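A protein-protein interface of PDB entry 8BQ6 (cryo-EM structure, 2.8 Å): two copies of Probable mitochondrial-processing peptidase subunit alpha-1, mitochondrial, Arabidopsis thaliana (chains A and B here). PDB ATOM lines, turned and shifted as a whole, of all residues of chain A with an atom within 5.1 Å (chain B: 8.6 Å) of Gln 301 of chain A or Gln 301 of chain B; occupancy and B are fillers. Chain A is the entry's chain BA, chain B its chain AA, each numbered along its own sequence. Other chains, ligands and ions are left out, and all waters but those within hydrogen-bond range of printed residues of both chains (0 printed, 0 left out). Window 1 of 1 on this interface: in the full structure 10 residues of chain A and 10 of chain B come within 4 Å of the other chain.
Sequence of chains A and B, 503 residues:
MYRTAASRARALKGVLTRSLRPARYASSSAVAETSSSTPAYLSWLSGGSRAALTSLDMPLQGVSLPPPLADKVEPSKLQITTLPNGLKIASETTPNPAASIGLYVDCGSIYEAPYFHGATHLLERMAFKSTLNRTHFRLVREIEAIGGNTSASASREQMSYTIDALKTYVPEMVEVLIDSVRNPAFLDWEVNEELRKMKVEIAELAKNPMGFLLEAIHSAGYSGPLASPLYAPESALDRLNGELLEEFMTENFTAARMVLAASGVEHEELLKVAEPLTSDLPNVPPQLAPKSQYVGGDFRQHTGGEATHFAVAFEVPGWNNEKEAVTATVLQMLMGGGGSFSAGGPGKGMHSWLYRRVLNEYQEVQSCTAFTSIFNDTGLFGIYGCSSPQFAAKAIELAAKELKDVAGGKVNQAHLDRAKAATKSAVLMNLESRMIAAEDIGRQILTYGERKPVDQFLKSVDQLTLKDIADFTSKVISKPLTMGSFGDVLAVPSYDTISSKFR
The backbone carbonyl oxygen (O) of Gln 301 of chain B sits at hydrogen-bond distance from the side-chain hydroxyl (OG1) of Thr 303 of chain B (3.3 Å).
The backbone NH of Gln 301 of chain A lies within hydrogen-bond range of the backbone carbonyl oxygen of Ser 485 of chain A, 3.4 Å away.
The backbone carbonyl oxygen (O) of Gln 301 of chain A sits at hydrogen-bond distance from the backbone NH (N) of Gly 487 of chain A (3.4 Å).
The backbone carbonyl oxygen of Gly 487 of chain A sits close to a ring nitrogen (ND1) of His 302 of chain A, at 3.4 Å.
Gln 301 of chain B touches Gln 301 of chain A.
His 302 of chain A touches Pro 233 of chain B (NE2 to CG, 3.8 Å).
Of the printed residues of chain B, Gln 301 of chain A touches Gln 301 (3.99 Å).
Printed residues of chain B within 4 Å of His 302 of chain A: Pro 233 (3.8 Å).
No residue of chain B comes within 4 Å of Gly 487 of chain A.
Of the printed residues of chain A, Pro 233 of chain B touches His 302.
Printed residues of chain A within 4 Å of Gln 301 of chain B: Gln 301.
The nearest printed residue of chain A that does not touch Gln 301 of chain B is Arg 300 of chain A (5.8 Å).
The nearest printed residue of chain A that does not touch Pro 233 of chain B is Thr 303 of chain A (4.7 Å).
Of the 10 printed residues of chain A, 2 touch a printed residue of chain B.
Printed residues of chain A that touch a printed residue of chain B: Gln 301 and His 302.
Gln 301 of chain B touches its own counterpart, Gln 301 of chain A.
10 positions are printed for both chains.
Of the 2 pairs that touch across the chains among the printed residues, 1 has its exchanged pair printed and touching as well.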
ATOM      1  N   PHE A 212       9.018  12.373  30.761  1.00  0.00           N
ATOM      2  CA  PHE A 212       9.646  12.019  29.495  1.00  0.00           C
ATOM      3  C   PHE A 212       9.769  13.235  28.589  1.00  0.00           C
ATOM      4  O   PHE A 212      10.795  13.431  27.927  1.00  0.00           O
ATOM      5  CB  PHE A 212       8.855  10.918  28.796  1.00  0.00           C
ATOM      6  CG  PHE A 212       9.470  10.484  27.509  1.00  0.00           C
ATOM      7  CD1 PHE A 212      10.617   9.713  27.509  1.00  0.00           C
ATOM      8  CD2 PHE A 212       8.937  10.885  26.299  1.00  0.00           C
ATOM      9  CE1 PHE A 212      11.203   9.325  26.328  1.00  0.00           C
ATOM     10  CE2 PHE A 212       9.528  10.504  25.114  1.00  0.00           C
ATOM     11  CZ  PHE A 212      10.652   9.717  25.126  1.00  0.00           C
ATOM     12  N   PHE A 299      11.004  17.982  18.960  1.00  0.00           N
ATOM     13  CA  PHE A 299      11.020  16.571  19.303  1.00  0.00           C
ATOM     14  C   PHE A 299       9.765  15.890  18.766  1.00  0.00           C
ATOM     15  O   PHE A 299       8.640  16.358  18.960  1.00  0.00           O
ATOM     16  CB  PHE A 299      11.130  16.386  20.819  1.00  0.00           C
ATOM     17  CG  PHE A 299      11.080  14.947  21.270  1.00  0.00           C
ATOM     18  CD1 PHE A 299      12.195  14.130  21.198  1.00  0.00           C
ATOM     19  CD2 PHE A 299       9.927  14.427  21.810  1.00  0.00           C
ATOM     20  CE1 PHE A 299      12.149  12.821  21.616  1.00  0.00           C
ATOM     21  CE2 PHE A 299       9.872  13.111  22.231  1.00  0.00           C
ATOM     22  CZ  PHE A 299      10.983  12.310  22.132  1.00  0.00           C
ATOM     23  N   ARG A 300       9.980  14.778  18.070  1.00  0.00           N
ATOM     24  CA  ARG A 300       8.891  13.955  17.567  1.00  0.00           C
ATOM     25  C   ARG A 300       9.201  12.502  17.873  1.00  0.00           C
ATOM     26  O   ARG A 300      10.357  12.080  17.785  1.00  0.00           O
ATOM     27  CB  ARG A 300       8.701  14.139  16.058  1.00  0.00           C
ATOM     28  CG  ARG A 300       8.239  15.519  15.658  1.00  0.00           C
ATOM     29  CD  ARG A 300       8.005  15.595  14.160  1.00  0.00           C
ATOM     30  NE  ARG A 300       7.578  16.922  13.727  1.00  0.00           N
ATOM     31  CZ  ARG A 300       6.331  17.373  13.772  1.00  0.00           C
ATOM     32  NH1 ARG A 300       5.327  16.603  14.158  1.00  0.00           N
ATOM     33  NH2 ARG A 300       6.082  18.625  13.402  1.00  0.00           N
ATOM     34  N   GLN A 301       8.168  11.746  18.231  1.00  0.00           N
ATOM     35  CA  GLN A 301       8.308  10.306  18.382  1.00  0.00           C
ATOM     36  C   GLN A 301       6.930   9.673  18.336  1.00  0.00           C
ATOM     37  O   GLN A 301       6.067  10.000  19.155  1.00  0.00           O
ATOM     38  CB  GLN A 301       9.018   9.941  19.684  1.00  0.00           C
ATOM     39  CG  GLN A 301      10.008   8.813  19.511  1.00  0.00           C
ATOM     40  CD  GLN A 301      10.271   8.081  20.800  1.00  0.00           C
ATOM     41  OE1 GLN A 301      10.171   8.655  21.882  1.00  0.00           O
ATOM     42  NE2 GLN A 301      10.606   6.800  20.698  1.00  0.00           N
ATOM     43  N   HIS A 302       6.736   8.767  17.384  1.00  0.00           N
ATOM     44  CA  HIS A 302       5.476   8.054  17.205  1.00  0.00           C
ATOM     45  C   HIS A 302       5.589   6.723  17.937  1.00  0.00           C
ATOM     46  O   HIS A 302       6.359   5.847  17.539  1.00  0.00           O
ATOM     47  CB  HIS A 302       5.177   7.851  15.724  1.00  0.00           C
ATOM     48  CG  HIS A 302       3.853   7.206  15.455  1.00  0.00           C
ATOM     49  ND1 HIS A 302       2.910   6.993  16.438  1.00  0.00           N
ATOM     50  CD2 HIS A 302       3.327   6.699  14.314  1.00  0.00           C
ATOM     51  CE1 HIS A 302       1.854   6.400  15.911  1.00  0.00           C
ATOM     52  NE2 HIS A 302       2.082   6.207  14.624  1.00  0.00           N
ATOM     53  N   THR A 303       4.826   6.576  19.018  1.00  0.00           N
ATOM     54  CA  THR A 303       4.780   5.331  19.771  1.00  0.00           C
ATOM     55  C   THR A 303       3.375   4.745  19.807  1.00  0.00           C
ATOM     56  O   THR A 303       3.082   3.890  20.649  1.00  0.00           O
ATOM     57  CB  THR A 303       5.304   5.545  21.191  1.00  0.00           C
ATOM     58  OG1 THR A 303       4.511   6.538  21.853  1.00  0.00           O
ATOM     59  CG2 THR A 303       6.751   6.010  21.156  1.00  0.00           C
ATOM     60  N   SER A 485       6.710  16.271  21.516  1.00  0.00           N
ATOM     61  CA  SER A 485       5.515  15.478  21.258  1.00  0.00           C
ATOM     62  C   SER A 485       5.830  14.000  21.396  1.00  0.00           C
ATOM     63  O   SER A 485       6.773  13.503  20.775  1.00  0.00           O
ATOM     64  CB  SER A 485       4.952  15.758  19.864  1.00  0.00           C
ATOM     65  OG  SER A 485       5.893  15.411  18.866  1.00  0.00           O
ATOM     66  N   PHE A 486       5.025  13.302  22.188  1.00  0.00           N
ATOM     67  CA  PHE A 486       5.174  11.871  22.386  1.00  0.00           C
ATOM     68  C   PHE A 486       3.821  11.203  22.213  1.00  0.00           C
ATOM     69  O   PHE A 486       2.783  11.794  22.520  1.00  0.00           O
ATOM     70  CB  PHE A 486       5.793  11.571  23.771  1.00  0.00           C
ATOM     71  CG  PHE A 486       5.676  10.126  24.213  1.00  0.00           C
ATOM     72  CD1 PHE A 486       6.805   9.339  24.280  1.00  0.00           C
ATOM     73  CD2 PHE A 486       4.479   9.590  24.667  1.00  0.00           C
ATOM     74  CE1 PHE A 486       6.747   8.031  24.705  1.00  0.00           C
ATOM     75  CE2 PHE A 486       4.408   8.277  25.089  1.00  0.00           C
ATOM     76  CZ  PHE A 486       5.548   7.498  25.113  1.00  0.00           C
ATOM     77  N   GLY A 487       3.846   9.966  21.726  1.00  0.00           N
ATOM     78  CA  GLY A 487       2.638   9.195  21.525  1.00  0.00           C
ATOM     79  C   GLY A 487       2.293   9.102  20.056  1.00  0.00           C
ATOM     80  O   GLY A 487       3.168   8.856  19.222  1.00  0.00           O
ATOM     81  N   VAL A 489       1.940  10.941  16.978  1.00  0.00           N
ATOM     82  CA  VAL A 489       2.399  12.223  16.460  1.00  0.00           C
ATOM     83  C   VAL A 489       2.049  12.382  14.984  1.00  0.00           C
ATOM     84  O   VAL A 489       2.503  13.331  14.334  1.00  0.00           O
ATOM     85  CB  VAL A 489       3.910  12.399  16.701  1.00  0.00           C
ATOM     86  CG1 VAL A 489       4.709  11.471  15.796  1.00  0.00           C
ATOM     87  CG2 VAL A 489       4.351  13.863  16.565  1.00  0.00           C
ATOM     88  N   ALA B 206      15.931  -1.873  12.794  1.00  0.00           N
ATOM     89  CA  ALA B 206      17.023  -1.034  13.271  1.00  0.00           C
ATOM     90  C   ALA B 206      18.398  -1.633  13.007  1.00  0.00           C
ATOM     91  O   ALA B 206      19.394  -1.072  13.473  1.00  0.00           O
ATOM     92  CB  ALA B 206      16.856  -0.763  14.766  1.00  0.00           C
ATOM     93  N   PHE B 212      15.971   1.954   7.602  1.00  0.00           N
ATOM     94  CA  PHE B 212      15.398   2.667   8.738  1.00  0.00           C
ATOM     95  C   PHE B 212      15.366   4.167   8.482  1.00  0.00           C
ATOM     96  O   PHE B 212      14.390   4.847   8.819  1.00  0.00           O
ATOM     97  CB  PHE B 212      16.189   2.361  10.009  1.00  0.00           C
ATOM     98  CG  PHE B 212      15.481   2.765  11.270  1.00  0.00           C
ATOM     99  CD1 PHE B 212      14.512   1.950  11.830  1.00  0.00           C
ATOM    100  CD2 PHE B 212      15.777   3.966  11.893  1.00  0.00           C
ATOM    101  CE1 PHE B 212      13.857   2.321  12.987  1.00  0.00           C
ATOM    102  CE2 PHE B 212      15.124   4.343  13.050  1.00  0.00           C
ATOM    103  CZ  PHE B 212      14.163   3.519  13.598  1.00  0.00           C
ATOM    104  N   LEU B 213      16.437   4.705   7.894  1.00  0.00           N
ATOM    105  CA  LEU B 213      16.496   6.138   7.638  1.00  0.00           C
ATOM    106  C   LEU B 213      15.621   6.528   6.460  1.00  0.00           C
ATOM    107  O   LEU B 213      15.153   7.669   6.375  1.00  0.00           O
ATOM    108  CB  LEU B 213      17.937   6.573   7.390  1.00  0.00           C
ATOM    109  CG  LEU B 213      18.642   7.123   8.623  1.00  0.00           C
ATOM    110  CD1 LEU B 213      20.113   7.350   8.337  1.00  0.00           C
ATOM    111  CD2 LEU B 213      17.969   8.406   9.055  1.00  0.00           C
ATOM    112  N   ALA B 216      12.243   6.813   7.961  1.00  0.00           N
ATOM    113  CA  ALA B 216      12.189   7.858   8.975  1.00  0.00           C
ATOM    114  C   ALA B 216      12.264   9.245   8.348  1.00  0.00           C
ATOM    115  O   ALA B 216      12.003  10.251   9.018  1.00  0.00           O
ATOM    116  CB  ALA B 216      13.305   7.656   9.995  1.00  0.00           C
ATOM    117  N   SER B 219       8.431   9.642   6.771  1.00  0.00           N
ATOM    118  CA  SER B 219       7.540  10.167   7.796  1.00  0.00           C
ATOM    119  C   SER B 219       7.804  11.646   8.046  1.00  0.00           C
ATOM    120  O   SER B 219       6.864  12.445   8.124  1.00  0.00           O
ATOM    121  CB  SER B 219       7.697   9.361   9.085  1.00  0.00           C
ATOM    122  OG  SER B 219       6.595   9.565   9.949  1.00  0.00           O
ATOM    123  N   PRO B 233       3.826   0.771  14.064  1.00  0.00           N
ATOM    124  CA  PRO B 233       4.313   0.526  15.426  1.00  0.00           C
ATOM    125  C   PRO B 233       3.513  -0.576  16.102  1.00  0.00           C
ATOM    126  O   PRO B 233       2.355  -0.840  15.775  1.00  0.00           O
ATOM    127  CB  PRO B 233       4.117   1.867  16.138  1.00  0.00           C
ATOM    128  CG  PRO B 233       3.129   2.603  15.325  1.00  0.00           C
ATOM    129  CD  PRO B 233       3.248   2.117  13.913  1.00  0.00           C
ATOM    130  N   ASP B 298      12.792  16.864  10.614  1.00  0.00           N
ATOM    131  CA  ASP B 298      13.973  16.223  11.159  1.00  0.00           C
ATOM    132  C   ASP B 298      13.543  14.961  11.888  1.00  0.00           C
ATOM    133  O   ASP B 298      12.486  14.929  12.525  1.00  0.00           O
ATOM    134  CB  ASP B 298      14.725  17.184  12.091  1.00  0.00           C
ATOM    135  CG  ASP B 298      16.044  16.625  12.591  1.00  0.00           C
ATOM    136  OD1 ASP B 298      16.414  15.489  12.226  1.00  0.00           O
ATOM    137  OD2 ASP B 298      16.731  17.350  13.337  1.00  0.00           O
ATOM    138  N   PHE B 299      14.347  13.912  11.756  1.00  0.00           N
ATOM    139  CA  PHE B 299      14.161  12.676  12.498  1.00  0.00           C
ATOM    140  C   PHE B 299      15.418  12.418  13.308  1.00  0.00           C
ATOM    141  O   PHE B 299      16.524  12.433  12.759  1.00  0.00           O
ATOM    142  CB  PHE B 299      13.889  11.496  11.566  1.00  0.00           C
ATOM    143  CG  PHE B 299      13.957  10.165  12.249  1.00  0.00           C
ATOM    144  CD1 PHE B 299      12.864   9.672  12.938  1.00  0.00           C
ATOM    145  CD2 PHE B 299      15.123   9.417  12.228  1.00  0.00           C
ATOM    146  CE1 PHE B 299      12.922   8.450  13.572  1.00  0.00           C
ATOM    147  CE2 PHE B 299      15.186   8.196  12.863  1.00  0.00           C
ATOM    148  CZ  PHE B 299      14.084   7.712  13.535  1.00  0.00           C
ATOM    149  N   ARG B 300      15.253  12.180  14.605  1.00  0.00           N
ATOM    150  CA  ARG B 300      16.406  11.976  15.477  1.00  0.00           C
ATOM    151  C   ARG B 300      16.039  10.922  16.509  1.00  0.00           C
ATOM    152  O   ARG B 300      15.021  11.054  17.195  1.00  0.00           O
ATOM    153  CB  ARG B 300      16.826  13.286  16.140  1.00  0.00           C
ATOM    154  CG  ARG B 300      17.472  14.245  15.160  1.00  0.00           C
ATOM    155  CD  ARG B 300      18.102  15.461  15.795  1.00  0.00           C
ATOM    156  NE  ARG B 300      18.754  16.248  14.757  1.00  0.00           N
ATOM    157  CZ  ARG B 300      19.326  17.429  14.939  1.00  0.00           C
ATOM    158  NH1 ARG B 300      19.362  18.005  16.130  1.00  0.00           N
ATOM    159  NH2 ARG B 300      19.876  18.046  13.899  1.00  0.00           N
ATOM    160  N   GLN B 301      16.851   9.874  16.604  1.00  0.00           N
ATOM    161  CA  GLN B 301      16.720   8.870  17.656  1.00  0.00           C
ATOM    162  C   GLN B 301      18.091   8.699  18.296  1.00  0.00           C
ATOM    163  O   GLN B 301      18.932   7.945  17.796  1.00  0.00           O
ATOM    164  CB  GLN B 301      16.185   7.549  17.112  1.00  0.00           C
ATOM    165  CG  GLN B 301      15.953   6.495  18.190  1.00  0.00           C
ATOM    166  CD  GLN B 301      14.798   6.841  19.119  1.00  0.00           C
ATOM    167  OE1 GLN B 301      14.014   7.751  18.845  1.00  0.00           O
ATOM    168  NE2 GLN B 301      14.696   6.117  20.228  1.00  0.00           N
ATOM    169  N   HIS B 302      18.315   9.400  19.402  1.00  0.00           N
ATOM    170  CA  HIS B 302      19.588   9.334  20.111  1.00  0.00           C
ATOM    171  C   HIS B 302      19.652   8.003  20.846  1.00  0.00           C
ATOM    172  O   HIS B 302      19.028   7.827  21.894  1.00  0.00           O
ATOM    173  CB  HIS B 302      19.731  10.508  21.071  1.00  0.00           C
ATOM    174  CG  HIS B 302      20.818  10.331  22.084  1.00  0.00           C
ATOM    175  ND1 HIS B 302      20.568  10.251  23.436  1.00  0.00           N
ATOM    176  CD2 HIS B 302      22.160  10.223  21.942  1.00  0.00           C
ATOM    177  CE1 HIS B 302      21.709  10.100  24.084  1.00  0.00           C
ATOM    178  NE2 HIS B 302      22.690  10.076  23.200  1.00  0.00           N
ATOM    179  N   THR B 303      20.399   7.053  20.287  1.00  0.00           N
ATOM    180  CA  THR B 303      20.573   5.753  20.915  1.00  0.00           C
ATOM    181  C   THR B 303      21.855   5.662  21.731  1.00  0.00           C
ATOM    182  O   THR B 303      21.914   4.875  22.682  1.00  0.00           O
ATOM    183  CB  THR B 303      20.573   4.646  19.850  1.00  0.00           C
ATOM    184  OG1 THR B 303      19.500   4.868  18.925  1.00  0.00           O
ATOM    185  CG2 THR B 303      20.383   3.282  20.493  1.00  0.00           C
ATOM    186  N   GLY B 304      22.866   6.457  21.395  1.00  0.00           N
ATOM    187  CA  GLY B 304      24.152   6.368  22.047  1.00  0.00           C
ATOM    188  C   GLY B 304      24.977   5.218  21.500  1.00  0.00           C
ATOM    189  O   GLY B 304      24.477   4.293  20.856  1.00  0.00           O
ATOM    190  N   THR B 308      27.389   6.516  13.800  1.00  0.00           N
ATOM    191  CA  THR B 308      26.331   7.445  13.434  1.00  0.00           C
ATOM    192  C   THR B 308      25.946   7.256  11.965  1.00  0.00           C
ATOM    193  O   THR B 308      26.736   6.789  11.142  1.00  0.00           O
ATOM    194  CB  THR B 308      26.791   8.882  13.714  1.00  0.00           C
ATOM    195  OG1 THR B 308      26.625   9.168  15.106  1.00  0.00           O
ATOM    196  CG2 THR B 308      26.009   9.917  12.910  1.00  0.00           C
ATOM    197  N   HIS B 309      24.693   7.577  11.650  1.00  0.00           N
ATOM    198  CA  HIS B 309      24.224   7.588  10.274  1.00  0.00           C
ATOM    199  C   HIS B 309      23.411   8.852  10.056  1.00  0.00           C
ATOM    200  O   HIS B 309      22.945   9.484  11.007  1.00  0.00           O
ATOM    201  CB  HIS B 309      23.405   6.334   9.960  1.00  0.00           C
ATOM    202  CG  HIS B 309      24.012   5.085  10.511  1.00  0.00           C
ATOM    203  ND1 HIS B 309      24.874   4.293   9.785  1.00  0.00           N
ATOM    204  CD2 HIS B 309      23.922   4.519  11.736  1.00  0.00           C
ATOM    205  CE1 HIS B 309      25.271   3.279  10.533  1.00  0.00           C
ATOM    206  NE2 HIS B 309      24.708   3.394  11.723  1.00  0.00           N
ATOM    207  N   GLY B 484      17.569  13.347   8.558  1.00  0.00           N
ATOM    208  CA  GLY B 484      17.418  12.175   9.394  1.00  0.00           C
ATOM    209  C   GLY B 484      18.746  11.703   9.942  1.00  0.00           C
ATOM    210  O   GLY B 484      19.706  11.544   9.186  1.00  0.00           O
ATOM    211  N   SER B 485      18.818  11.487  11.254  1.00  0.00           N
ATOM    212  CA  SER B 485      20.007  10.954  11.900  1.00  0.00           C
ATOM    213  C   SER B 485      19.615   9.790  12.799  1.00  0.00           C
ATOM    214  O   SER B 485      18.534   9.783  13.394  1.00  0.00           O
ATOM    215  CB  SER B 485      20.738  12.026  12.719  1.00  0.00           C
ATOM    216  OG  SER B 485      20.834  13.245  12.002  1.00  0.00           O
ATOM    217  N   PHE B 486      20.502   8.800  12.881  1.00  0.00           N
ATOM    218  CA  PHE B 486      20.265   7.601  13.679  1.00  0.00           C
ATOM    219  C   PHE B 486      21.574   7.204  14.344  1.00  0.00           C
ATOM    220  O   PHE B 486      22.635   7.290  13.719  1.00  0.00           O
ATOM    221  CB  PHE B 486      19.734   6.461  12.806  1.00  0.00           C
ATOM    222  CG  PHE B 486      19.368   5.225  13.575  1.00  0.00           C
ATOM    223  CD1 PHE B 486      18.275   5.217  14.423  1.00  0.00           C
ATOM    224  CD2 PHE B 486      20.125   4.071  13.455  1.00  0.00           C
ATOM    225  CE1 PHE B 486      17.939   4.077  15.134  1.00  0.00           C
ATOM    226  CE2 PHE B 486      19.797   2.932  14.162  1.00  0.00           C
ATOM    227  CZ  PHE B 486      18.703   2.934  15.003  1.00  0.00           C
ATOM    228  N   GLY B 487      21.505   6.773  15.601  1.00  0.00           N
ATOM    229  CA  GLY B 487      22.701   6.370  16.315  1.00  0.00           C
ATOM    230  C   GLY B 487      23.124   7.359  17.382  1.00  0.00           C
ATOM    231  O   GLY B 487      22.438   7.513  18.396  1.00  0.00           O
ATOM    232  N   ASP B 488      24.257   8.025  17.172  1.00  0.00           N
ATOM    233  CA  ASP B 488      24.735   9.070  18.072  1.00  0.00           C
ATOM    234  C   ASP B 488      24.400  10.410  17.437  1.00  0.00           C
ATOM    235  O   ASP B 488      25.028  10.808  16.452  1.00  0.00           O
ATOM    236  CB  ASP B 488      26.238   8.956  18.305  1.00  0.00           C
ATOM    237  CG  ASP B 488      26.633   7.635  18.900  1.00  0.00           C
ATOM    238  OD1 ASP B 488      27.846   7.414  19.071  1.00  0.00           O
ATOM    239  OD2 ASP B 488      25.736   6.813  19.176  1.00  0.00           O
ATOM    240  N   VAL B 489      23.412  11.106  17.998  1.00  0.00           N
ATOM    241  CA  VAL B 489      22.961  12.368  17.429  1.00  0.00           C
ATOM    242  C   VAL B 489      23.335  13.555  18.304  1.00  0.00           C
ATOM    243  O   VAL B 489      22.953  14.693  17.994  1.00  0.00           O
ATOM    244  CB  VAL B 489      21.442  12.325  17.174  1.00  0.00           C
ATOM    245  CG1 VAL B 489      21.037  13.347  16.117  1.00  0.00           C
ATOM    246  CG2 VAL B 489      21.019  10.917  16.768  1.00  0.00           C
ATOM    247  N   LEU B 490      24.074  13.325  19.389  1.00  0.00           N
ATOM    248  CA  LEU B 490      24.499  14.431  20.239  1.00  0.00           C
ATOM    249  C   LEU B 490      25.448  15.363  19.499  1.00  0.00           C
ATOM    250  O   LEU B 490      25.297  16.589  19.560  1.00  0.00           O
ATOM    251  CB  LEU B 490      25.156  13.894  21.509  1.00  0.00           C
ATOM    252  CG  LEU B 490      24.286  12.947  22.331  1.00  0.00           C
ATOM    253  CD1 LEU B 490      25.126  12.197  23.347  1.00  0.00           C
ATOM    254  CD2 LEU B 490      23.184  13.731  23.015  1.00  0.00           C
